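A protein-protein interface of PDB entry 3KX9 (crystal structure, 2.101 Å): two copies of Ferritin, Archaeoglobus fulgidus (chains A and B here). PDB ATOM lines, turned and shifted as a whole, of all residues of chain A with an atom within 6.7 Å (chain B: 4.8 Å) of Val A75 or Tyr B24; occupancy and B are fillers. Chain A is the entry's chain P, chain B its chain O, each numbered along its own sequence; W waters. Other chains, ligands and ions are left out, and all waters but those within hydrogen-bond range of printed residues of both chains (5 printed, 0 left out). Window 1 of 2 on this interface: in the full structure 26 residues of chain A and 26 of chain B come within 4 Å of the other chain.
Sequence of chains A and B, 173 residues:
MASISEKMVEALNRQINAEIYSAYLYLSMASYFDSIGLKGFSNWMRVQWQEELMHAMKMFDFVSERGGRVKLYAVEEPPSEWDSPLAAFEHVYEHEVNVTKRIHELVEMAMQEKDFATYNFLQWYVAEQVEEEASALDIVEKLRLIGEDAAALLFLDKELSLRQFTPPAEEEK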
ATOM      1  N   ILE A  16      12.743  11.747 -28.315  1.00  0.00           N
ATOM      2  CA  ILE A  16      12.742  10.698 -29.343  1.00  0.00           C
ATOM      3  C   ILE A  16      12.561   9.336 -28.679  1.00  0.00           C
ATOM      4  O   ILE A  16      11.755   8.526 -29.120  1.00  0.00           O
ATOM      5  CB  ILE A  16      14.046  10.707 -30.195  1.00  0.00           C
ATOM      6  CG1 ILE A  16      14.104  11.975 -31.060  1.00  0.00           C
ATOM      7  CG2 ILE A  16      14.129   9.460 -31.087  1.00  0.00           C
ATOM      8  CD1 ILE A  16      15.459  12.204 -31.732  1.00  0.00           C
ATOM      9  N   ASN A  17      13.314   9.099 -27.608  1.00  0.00           N
ATOM     10  CA  ASN A  17      13.166   7.869 -26.854  1.00  0.00           C
ATOM     11  C   ASN A  17      11.736   7.736 -26.341  1.00  0.00           C
ATOM     12  O   ASN A  17      11.134   6.670 -26.437  1.00  0.00           O
ATOM     13  CB  ASN A  17      14.170   7.798 -25.695  1.00  0.00           C
ATOM     14  CG  ASN A  17      14.166   6.439 -25.011  1.00  0.00           C
ATOM     15  OD1 ASN A  17      14.758   5.465 -25.506  1.00  0.00           O
ATOM     16  ND2 ASN A  17      13.475   6.354 -23.883  1.00  0.00           N
ATOM     17  N   ILE A  20       9.355   6.727 -29.171  1.00  0.00           N
ATOM     18  CA  ILE A  20       9.527   5.341 -29.581  1.00  0.00           C
ATOM     19  C   ILE A  20       8.961   4.431 -28.496  1.00  0.00           C
ATOM     20  O   ILE A  20       8.356   3.409 -28.793  1.00  0.00           O
ATOM     21  CB  ILE A  20      10.993   4.994 -29.900  1.00  0.00           C
ATOM     22  CG1 ILE A  20      11.421   5.704 -31.188  1.00  0.00           C
ATOM     23  CG2 ILE A  20      11.148   3.487 -30.074  1.00  0.00           C
ATOM     24  CD1 ILE A  20      12.904   5.625 -31.469  1.00  0.00           C
ATOM     25  N   TYR A  21       9.134   4.818 -27.241  1.00  0.00           N
ATOM     26  CA  TYR A  21       8.506   4.060 -26.159  1.00  0.00           C
ATOM     27  C   TYR A  21       6.985   4.086 -26.307  1.00  0.00           C
ATOM     28  O   TYR A  21       6.327   3.074 -26.077  1.00  0.00           O
ATOM     29  CB  TYR A  21       8.912   4.556 -24.759  1.00  0.00           C
ATOM     30  CG  TYR A  21       8.118   3.833 -23.693  1.00  0.00           C
ATOM     31  CD1 TYR A  21       8.444   2.532 -23.314  1.00  0.00           C
ATOM     32  CD2 TYR A  21       7.007   4.421 -23.122  1.00  0.00           C
ATOM     33  CE1 TYR A  21       7.688   1.851 -22.371  1.00  0.00           C
ATOM     34  CE2 TYR A  21       6.243   3.753 -22.189  1.00  0.00           C
ATOM     35  CZ  TYR A  21       6.589   2.475 -21.812  1.00  0.00           C
ATOM     36  OH  TYR A  21       5.823   1.838 -20.884  1.00  0.00           O
ATOM     37  N   SER A  22       6.423   5.230 -26.704  1.00  0.00           N
ATOM     38  CA  SER A  22       4.971   5.307 -26.881  1.00  0.00           C
ATOM     39  C   SER A  22       4.509   4.304 -27.929  1.00  0.00           C
ATOM     40  O   SER A  22       3.542   3.576 -27.719  1.00  0.00           O
ATOM     41  CB  SER A  22       4.522   6.715 -27.270  1.00  0.00           C
ATOM     42  OG  SER A  22       4.688   7.613 -26.186  1.00  0.00           O
ATOM     43  N   TYR A  24       5.961   1.658 -28.666  1.00  0.00           N
ATOM     44  CA  TYR A  24       6.208   0.320 -28.148  1.00  0.00           C
ATOM     45  C   TYR A  24       5.075  -0.124 -27.215  1.00  0.00           C
ATOM     46  O   TYR A  24       4.646  -1.284 -27.237  1.00  0.00           O
ATOM     47  CB  TYR A  24       7.575   0.290 -27.444  1.00  0.00           C
ATOM     48  CG  TYR A  24       8.285  -1.065 -27.390  1.00  0.00           C
ATOM     49  CD1 TYR A  24       8.268  -1.937 -28.477  1.00  0.00           C
ATOM     50  CD2 TYR A  24       9.016  -1.442 -26.261  1.00  0.00           C
ATOM     51  CE1 TYR A  24       8.942  -3.176 -28.428  1.00  0.00           C
ATOM     52  CE2 TYR A  24       9.689  -2.671 -26.199  1.00  0.00           C
ATOM     53  CZ  TYR A  24       9.647  -3.529 -27.284  1.00  0.00           C
ATOM     54  OH  TYR A  24      10.319  -4.733 -27.233  1.00  0.00           O
ATOM     55  N   LYS A  71      21.374  10.419 -30.472  1.00  0.00           N
ATOM     56  CA  LYS A  71      21.858   9.279 -29.712  1.00  0.00           C
ATOM     57  C   LYS A  71      20.652   8.498 -29.237  1.00  0.00           C
ATOM     58  O   LYS A  71      19.730   9.075 -28.645  1.00  0.00           O
ATOM     59  CB  LYS A  71      22.672   9.743 -28.507  1.00  0.00           C
ATOM     60  CG  LYS A  71      23.857   8.846 -28.227  1.00  0.00           C
ATOM     61  CD  LYS A  71      23.800   8.251 -26.841  1.00  0.00           C
ATOM     62  CE  LYS A  71      25.043   7.397 -26.563  1.00  0.00           C
ATOM     63  NZ  LYS A  71      25.227   6.315 -27.572  1.00  0.00           N
ATOM     64  N   LEU A  72      20.650   7.195 -29.509  1.00  0.00           N
ATOM     65  CA  LEU A  72      19.495   6.361 -29.184  1.00  0.00           C
ATOM     66  C   LEU A  72      19.715   5.645 -27.857  1.00  0.00           C
ATOM     67  O   LEU A  72      20.775   5.059 -27.621  1.00  0.00           O
ATOM     68  CB  LEU A  72      19.218   5.352 -30.302  1.00  0.00           C
ATOM     69  CG  LEU A  72      18.904   5.912 -31.698  1.00  0.00           C
ATOM     70  CD1 LEU A  72      18.917   4.798 -32.745  1.00  0.00           C
ATOM     71  CD2 LEU A  72      17.573   6.670 -31.734  1.00  0.00           C
ATOM     72  N   TYR A  73      18.708   5.704 -26.992  1.00  0.00           N
ATOM     73  CA  TYR A  73      18.779   5.095 -25.674  1.00  0.00           C
ATOM     74  C   TYR A  73      17.912   3.842 -25.649  1.00  0.00           C
ATOM     75  O   TYR A  73      17.132   3.619 -26.564  1.00  0.00           O
ATOM     76  CB  TYR A  73      18.301   6.090 -24.614  1.00  0.00           C
ATOM     77  CG  TYR A  73      19.083   7.374 -24.611  1.00  0.00           C
ATOM     78  CD1 TYR A  73      18.485   8.579 -24.975  1.00  0.00           C
ATOM     79  CD2 TYR A  73      20.428   7.383 -24.275  1.00  0.00           C
ATOM     80  CE1 TYR A  73      19.207   9.763 -24.981  1.00  0.00           C
ATOM     81  CE2 TYR A  73      21.154   8.555 -24.282  1.00  0.00           C
ATOM     82  CZ  TYR A  73      20.539   9.743 -24.634  1.00  0.00           C
ATOM     83  OH  TYR A  73      21.267  10.912 -24.638  1.00  0.00           O
ATOM     84  N   ALA A  74      18.058   3.030 -24.603  1.00  0.00           N
ATOM     85  CA  ALA A  74      17.304   1.791 -24.486  1.00  0.00           C
ATOM     86  C   ALA A  74      15.816   2.113 -24.494  1.00  0.00           C
ATOM     87  O   ALA A  74      15.409   3.122 -23.945  1.00  0.00           O
ATOM     88  CB  ALA A  74      17.689   1.052 -23.197  1.00  0.00           C
ATOM     89  N   VAL A  75      15.007   1.271 -25.134  1.00  0.00           N
ATOM     90  CA  VAL A  75      13.563   1.436 -25.065  1.00  0.00           C
ATOM     91  C   VAL A  75      13.036   0.544 -23.951  1.00  0.00           C
ATOM     92  O   VAL A  75      13.173  -0.682 -24.013  1.00  0.00           O
ATOM     93  CB  VAL A  75      12.853   1.081 -26.379  1.00  0.00           C
ATOM     94  CG1 VAL A  75      11.355   1.443 -26.280  1.00  0.00           C
ATOM     95  CG2 VAL A  75      13.519   1.785 -27.558  1.00  0.00           C
ATOM     96  N   GLU A  76      12.449   1.176 -22.934  1.00  0.00           N
ATOM     97  CA  GLU A  76      11.974   0.490 -21.738  1.00  0.00           C
ATOM     98  C   GLU A  76      10.891  -0.551 -22.018  1.00  0.00           C
ATOM     99  O   GLU A  76      10.096  -0.420 -22.951  1.00  0.00           O
ATOM    100  CB  GLU A  76      11.419   1.514 -20.725  1.00  0.00           C
ATOM    101  CG  GLU A  76      12.311   2.699 -20.473  1.00  0.00           C
ATOM    102  CD  GLU A  76      13.439   2.373 -19.531  1.00  0.00           C
ATOM    103  OE1 GLU A  76      13.560   1.179 -19.170  1.00  0.00           O
ATOM    104  OE2 GLU A  76      14.185   3.306 -19.140  1.00  0.00           O
ATOM    105  N   GLU A  77      10.853  -1.573 -21.173  1.00  0.00           N
ATOM    106  CA  GLU A  77       9.862  -2.621 -21.267  1.00  0.00           C
ATOM    107  C   GLU A  77       8.464  -2.104 -20.881  1.00  0.00           C
ATOM    108  O   GLU A  77       8.269  -1.545 -19.794  1.00  0.00           O
ATOM    109  CB  GLU A  77      10.290  -3.793 -20.375  1.00  0.00           C
ATOM    110  CG  GLU A  77       9.329  -4.985 -20.388  1.00  0.00           C
ATOM    111  CD  GLU A  77       9.847  -6.121 -19.540  1.00  0.00           C
ATOM    112  OE1 GLU A  77      10.995  -6.017 -19.049  1.00  0.00           O
ATOM    113  OE2 GLU A  77       9.120  -7.115 -19.370  1.00  0.00           O
ATOM    114  N   PRO A  78       7.483  -2.256 -21.778  1.00  0.00           N
ATOM    115  CA  PRO A  78       6.150  -1.732 -21.429  1.00  0.00           C
ATOM    116  C   PRO A  78       5.314  -2.713 -20.589  1.00  0.00           C
ATOM    117  O   PRO A  78       5.690  -3.873 -20.454  1.00  0.00           O
ATOM    118  CB  PRO A  78       5.501  -1.503 -22.789  1.00  0.00           C
ATOM    119  CG  PRO A  78       6.122  -2.547 -23.674  1.00  0.00           C
ATOM    120  CD  PRO A  78       7.553  -2.727 -23.173  1.00  0.00           C
ATOM    121  N   ILE B  20      13.684  -6.331 -33.537  1.00  0.00           N
ATOM    122  CA  ILE B  20      13.473  -4.915 -33.240  1.00  0.00           C
ATOM    123  C   ILE B  20      14.805  -4.246 -32.874  1.00  0.00           C
ATOM    124  O   ILE B  20      15.083  -3.124 -33.301  1.00  0.00           O
ATOM    125  CB  ILE B  20      12.412  -4.712 -32.154  1.00  0.00           C
ATOM    126  CG1 ILE B  20      11.035  -5.127 -32.685  1.00  0.00           C
ATOM    127  CG2 ILE B  20      12.384  -3.263 -31.710  1.00  0.00           C
ATOM    128  CD1 ILE B  20       9.952  -5.186 -31.595  1.00  0.00           C
ATOM    129  N   TYR B  21      15.653  -4.946 -32.126  1.00  0.00           N
ATOM    130  CA  TYR B  21      17.010  -4.420 -31.883  1.00  0.00           C
ATOM    131  C   TYR B  21      17.805  -4.229 -33.188  1.00  0.00           C
ATOM    132  O   TYR B  21      18.479  -3.217 -33.363  1.00  0.00           O
ATOM    133  CB  TYR B  21      17.819  -5.278 -30.900  1.00  0.00           C
ATOM    134  CG  TYR B  21      19.235  -4.743 -30.778  1.00  0.00           C
ATOM    135  CD1 TYR B  21      19.498  -3.577 -30.065  1.00  0.00           C
ATOM    136  CD2 TYR B  21      20.293  -5.364 -31.435  1.00  0.00           C
ATOM    137  CE1 TYR B  21      20.790  -3.059 -29.988  1.00  0.00           C
ATOM    138  CE2 TYR B  21      21.585  -4.860 -31.361  1.00  0.00           C
ATOM    139  CZ  TYR B  21      21.824  -3.707 -30.638  1.00  0.00           C
ATOM    140  OH  TYR B  21      23.096  -3.204 -30.555  1.00  0.00           O
ATOM    141  N   SER B  22      17.718  -5.185 -34.112  1.00  0.00           N
ATOM    142  CA  SER B  22      18.411  -5.010 -35.387  1.00  0.00           C
ATOM    143  C   SER B  22      17.955  -3.714 -36.042  1.00  0.00           C
ATOM    144  O   SER B  22      18.783  -2.923 -36.501  1.00  0.00           O
ATOM    145  CB  SER B  22      18.204  -6.209 -36.327  1.00  0.00           C
ATOM    146  OG  SER B  22      18.625  -7.417 -35.713  1.00  0.00           O
ATOM    147  N   ALA B  23      16.640  -3.482 -36.061  1.00  0.00           N
ATOM    148  CA  ALA B  23      16.113  -2.260 -36.658  1.00  0.00           C
ATOM    149  C   ALA B  23      16.749  -1.028 -36.027  1.00  0.00           C
ATOM    150  O   ALA B  23      17.071  -0.056 -36.718  1.00  0.00           O
ATOM    151  CB  ALA B  23      14.581  -2.208 -36.505  1.00  0.00           C
ATOM    152  N   TYR B  24      16.910  -1.085 -34.704  1.00  0.00           N
ATOM    153  CA  TYR B  24      17.344   0.041 -33.879  1.00  0.00           C
ATOM    154  C   TYR B  24      18.830   0.313 -34.092  1.00  0.00           C
ATOM    155  O   TYR B  24      19.279   1.460 -34.087  1.00  0.00           O
ATOM    156  CB  TYR B  24      17.102  -0.300 -32.407  1.00  0.00           C
ATOM    157  CG  TYR B  24      16.852   0.883 -31.504  1.00  0.00           C
ATOM    158  CD1 TYR B  24      16.080   1.969 -31.930  1.00  0.00           C
ATOM    159  CD2 TYR B  24      17.334   0.889 -30.208  1.00  0.00           C
ATOM    160  CE1 TYR B  24      15.832   3.046 -31.083  1.00  0.00           C
ATOM    161  CE2 TYR B  24      17.102   1.954 -29.361  1.00  0.00           C
ATOM    162  CZ  TYR B  24      16.347   3.023 -29.799  1.00  0.00           C
ATOM    163  OH  TYR B  24      16.128   4.068 -28.943  1.00  0.00           O
ATOM    164  N   LEU B  25      19.585  -0.758 -34.285  1.00  0.00           N
ATOM    165  CA  LEU B  25      20.999  -0.650 -34.600  1.00  0.00           C
ATOM    166  C   LEU B  25      21.139   0.056 -35.943  1.00  0.00           C
ATOM    167  O   LEU B  25      21.940   0.973 -36.103  1.00  0.00           O
ATOM    168  CB  LEU B  25      21.621  -2.043 -34.661  1.00  0.00           C
ATOM    169  CG  LEU B  25      23.029  -2.075 -35.269  1.00  0.00           C
ATOM    170  CD1 LEU B  25      24.012  -1.375 -34.325  1.00  0.00           C
ATOM    171  CD2 LEU B  25      23.473  -3.502 -35.588  1.00  0.00           C
ATOM    172  N   TYR B  26      20.330  -0.348 -36.912  1.00  0.00           N
ATOM    173  CA  TYR B  26      20.363   0.330 -38.207  1.00  0.00           C
ATOM    174  C   TYR B  26      19.967   1.809 -38.116  1.00  0.00           C
ATOM    175  O   TYR B  26      20.594   2.653 -38.753  1.00  0.00           O
ATOM    176  CB  TYR B  26      19.574  -0.451 -39.258  1.00  0.00           C
ATOM    177  CG  TYR B  26      20.120  -1.861 -39.386  1.00  0.00           C
ATOM    178  CD1 TYR B  26      21.477  -2.101 -39.223  1.00  0.00           C
ATOM    179  CD2 TYR B  26      19.293  -2.947 -39.648  1.00  0.00           C
ATOM    180  CE1 TYR B  26      22.001  -3.371 -39.320  1.00  0.00           C
ATOM    181  CE2 TYR B  26      19.813  -4.234 -39.743  1.00  0.00           C
ATOM    182  CZ  TYR B  26      21.169  -4.433 -39.581  1.00  0.00           C
ATOM    183  OH  TYR B  26      21.727  -5.691 -39.678  1.00  0.00           O
ATOM    184  N   LEU B  27      18.957   2.126 -37.307  1.00  0.00           N
ATOM    185  CA  LEU B  27      18.577   3.522 -37.098  1.00  0.00           C
ATOM    186  C   LEU B  27      19.749   4.318 -36.505  1.00  0.00           C
ATOM    187  O   LEU B  27      19.972   5.483 -36.852  1.00  0.00           O
ATOM    188  CB  LEU B  27      17.339   3.625 -36.188  1.00  0.00           C
ATOM    189  CG  LEU B  27      16.774   5.033 -35.980  1.00  0.00           C
ATOM    190  CD1 LEU B  27      16.288   5.623 -37.305  1.00  0.00           C
ATOM    191  CD2 LEU B  27      15.655   5.037 -34.942  1.00  0.00           C
ATOM    192  N   SER B  28      20.491   3.687 -35.605  1.00  0.00           N
ATOM    193  CA  SER B  28      21.649   4.323 -35.014  1.00  0.00           C
ATOM    194  C   SER B  28      22.696   4.607 -36.097  1.00  0.00           C
ATOM    195  O   SER B  28      23.321   5.658 -36.104  1.00  0.00           O
ATOM    196  CB  SER B  28      22.237   3.450 -33.904  1.00  0.00           C
ATOM    197  OG  SER B  28      23.209   4.182 -33.181  1.00  0.00           O
ATOM    198  N   TRP B  49      16.013  -0.422 -41.358  1.00  0.00           N
ATOM    199  CA  TRP B  49      15.242  -0.304 -40.111  1.00  0.00           C
ATOM    200  C   TRP B  49      13.760  -0.638 -40.341  1.00  0.00           C
ATOM    201  O   TRP B  49      13.155  -1.414 -39.590  1.00  0.00           O
ATOM    202  CB  TRP B  49      15.493   1.078 -39.468  1.00  0.00           C
ATOM    203  CG  TRP B  49      14.303   1.861 -38.948  1.00  0.00           C
ATOM    204  CD1 TRP B  49      13.481   2.682 -39.674  1.00  0.00           C
ATOM    205  CD2 TRP B  49      13.851   1.950 -37.582  1.00  0.00           C
ATOM    206  NE1 TRP B  49      12.524   3.244 -38.852  1.00  0.00           N
ATOM    207  CE2 TRP B  49      12.735   2.819 -37.565  1.00  0.00           C
ATOM    208  CE3 TRP B  49      14.271   1.366 -36.376  1.00  0.00           C
ATOM    209  CZ2 TRP B  49      12.028   3.116 -36.390  1.00  0.00           C
ATOM    210  CZ3 TRP B  49      13.555   1.659 -35.199  1.00  0.00           C
ATOM    211  CH2 TRP B  49      12.454   2.526 -35.220  1.00  0.00           C
ATOM    212  N   TYR B  73      10.056  -6.976 -24.600  1.00  0.00           N
ATOM    213  CA  TYR B  73      11.154  -6.733 -23.662  1.00  0.00           C
ATOM    214  C   TYR B  73      11.863  -5.417 -23.969  1.00  0.00           C
ATOM    215  O   TYR B  73      11.692  -4.853 -25.049  1.00  0.00           O
ATOM    216  CB  TYR B  73      12.171  -7.885 -23.699  1.00  0.00           C
ATOM    217  CG  TYR B  73      11.577  -9.218 -23.322  1.00  0.00           C
ATOM    218  CD1 TYR B  73      11.422 -10.219 -24.269  1.00  0.00           C
ATOM    219  CD2 TYR B  73      11.141  -9.467 -22.020  1.00  0.00           C
ATOM    220  CE1 TYR B  73      10.863 -11.443 -23.934  1.00  0.00           C
ATOM    221  CE2 TYR B  73      10.573 -10.682 -21.680  1.00  0.00           C
ATOM    222  CZ  TYR B  73      10.444 -11.671 -22.644  1.00  0.00           C
ATOM    223  OH  TYR B  73       9.888 -12.896 -22.324  1.00  0.00           O
ATOM    224  N   ALA B  74      12.655  -4.922 -23.019  1.00  0.00           N
ATOM    225  CA  ALA B  74      13.419  -3.702 -23.260  1.00  0.00           C
ATOM    226  C   ALA B  74      14.231  -3.865 -24.544  1.00  0.00           C
ATOM    227  O   ALA B  74      14.721  -4.951 -24.842  1.00  0.00           O
ATOM    228  CB  ALA B  74      14.335  -3.384 -22.085  1.00  0.00           C
ATOM    229  N   VAL B  75      14.346  -2.790 -25.315  1.00  0.00           N
ATOM    230  CA  VAL B  75      15.239  -2.797 -26.467  1.00  0.00           C
ATOM    231  C   VAL B  75      16.526  -2.094 -26.051  1.00  0.00           C
ATOM    232  O   VAL B  75      16.511  -0.915 -25.707  1.00  0.00           O
ATOM    233  CB  VAL B  75      14.628  -2.077 -27.675  1.00  0.00           C
ATOM    234  CG1 VAL B  75      15.603  -2.111 -28.857  1.00  0.00           C
ATOM    235  CG2 VAL B  75      13.293  -2.714 -28.048  1.00  0.00           C
ATOM    236  N   GLU B  76      17.635  -2.823 -26.074  1.00  0.00           N
ATOM    237  CA  GLU B  76      18.886  -2.296 -25.539  1.00  0.00           C
ATOM    238  C   GLU B  76      19.452  -1.182 -26.403  1.00  0.00           C
ATOM    239  O   GLU B  76      19.136  -1.079 -27.589  1.00  0.00           O
ATOM    240  CB  GLU B  76      19.902  -3.422 -25.322  1.00  0.00           C
ATOM    241  CG  GLU B  76      20.534  -3.991 -26.574  1.00  0.00           C
ATOM    242  CD  GLU B  76      21.603  -5.036 -26.234  1.00  0.00           C
ATOM    243  OE1 GLU B  76      21.459  -6.209 -26.649  1.00  0.00           O
ATOM    244  OE2 GLU B  76      22.580  -4.685 -25.532  1.00  0.00           O
ATOM    245  N   PRO B  78      21.855   0.604 -28.753  1.00  0.00           N
ATOM    246  CA  PRO B  78      22.833   0.156 -29.756  1.00  0.00           C
ATOM    247  C   PRO B  78      24.058   1.053 -29.747  1.00  0.00           C
ATOM    248  O   PRO B  78      23.958   2.187 -29.285  1.00  0.00           O
ATOM    249  CB  PRO B  78      22.103   0.376 -31.075  1.00  0.00           C
ATOM    250  CG  PRO B  78      21.147   1.532 -30.792  1.00  0.00           C
ATOM    251  CD  PRO B  78      20.892   1.574 -29.306  1.00  0.00           C
HETATM  252  O   HOH W   1      13.155  -6.200 -20.632  1.00  0.00           O
HETATM  253  O   HOH W   2      23.228   4.746 -28.908  1.00  0.00           O
HETATM  254  O   HOH W   3      10.714  -7.372 -27.241  1.00  0.00           O
HETATM  255  O   HOH W   4      16.153   6.684 -27.984  1.00  0.00           O
HETATM  256  O   HOH W   5      22.633   6.295 -31.527  1.00  0.00           O
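Of the 14 printed residues of chain A, 8 touch a printed residue of chain B.
Printed residues of chain B within 4 Å of Asn A17: Tyr B24 (3.95 Å). Of the printed residues of chain B, Tyr A24 touches Ile B20 (3.9 Å), Tyr B73 (2.6 Å) and Val B75 (3.7 Å). Of the printed residues of chain B, Tyr A73 touches Tyr B24 (2.6 Å). Of chain B, only Tyr B24 (3.7 Å), Ala B74 (3.1 Å) and Val B75 (2.7 Å) come within 4 Å of Val A75. Printed residues of chain B within 4 Å of Glu A77: Ala B74 (3.7 Å). Tyr B24 touches five residues of chain A. Printed residues of chain A within 4 Å of Val B75: Tyr A24 (3.7 Å), Ala A74 (3.1 Å) and Val A75 (2.7 Å). The nearest residue of chain B that does not touch Val A75 is Tyr B73 (4.5 Å).
The side-chain amide oxygen (OD1) of Asn A17 sits close to the backbone carbonyl oxygen (O) of Tyr A73 (3.2 Å). OD1 of Asn A17 lies close to O of Ala A74, 2.9 Å away.
Water W3 bridges OH of Tyr A24 and N of Tyr B73. Water W1 bridges OE1 of Glu A77 (2.7 Å) and N of Ala B74 (2.8 Å). Water W2 lies within hydrogen-bond range of O of Pro B78 (2.7 Å), O of Leu A72 (2.8 Å) and NZ of Lys A71 (2.9 Å). Water W5 lies within hydrogen-bond range of the side-chain hydroxyl of Ser B28 (2.7 Å) and the backbone NH of Leu A72 (3.0 Å). Water W4 lies within hydrogen-bond range of OH of Tyr B24, N of Tyr A73 and OD1 of Asn A17.
The side-chain hydroxyl of Tyr B24 is in hydrogen-bond range of the backbone carbonyl oxygen of Tyr A73 (2.6 Å). O of Tyr B73 lies within hydrogen-bond range of OH of Tyr A24 (2.6 Å). The backbone carbonyl oxygen (O) of Val B75 sits at hydrogen-bond distance from the backbone NH (N) of Val A75 (2.7 Å).
Tyr A24 touches Tyr B73, and with the chains exchanged Tyr A73 touches Tyr B24. Tyr A24 touches Val B75, and with the chains exchanged Val A75 touches Tyr B24. Ala A74 touches Val B75, and with the chains exchanged Val A75 touches Ala B74. Val B75 touches its own counterpart, Val A75. 9 positions are printed for both chains. Of the 15 pairs that touch across the chains among the printed residues, 9 have their exchanged pair printed and touching as well.
Among the printed residues, merely in contact across the chains: Asn A17 with Tyr B24, Ile A20 with Tyr B24, Tyr A24 with Ile B20, Tyr A24 with Val B75, Leu A72 with Tyr B24, Leu A72 with Leu B27, Leu A72 with Ser B28, Leu A72 with Pro B78, Ala A74 with Val B75, Val A75 with Tyr B24, Val A75 with Ala B74 and Glu A77 with Ala B74.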
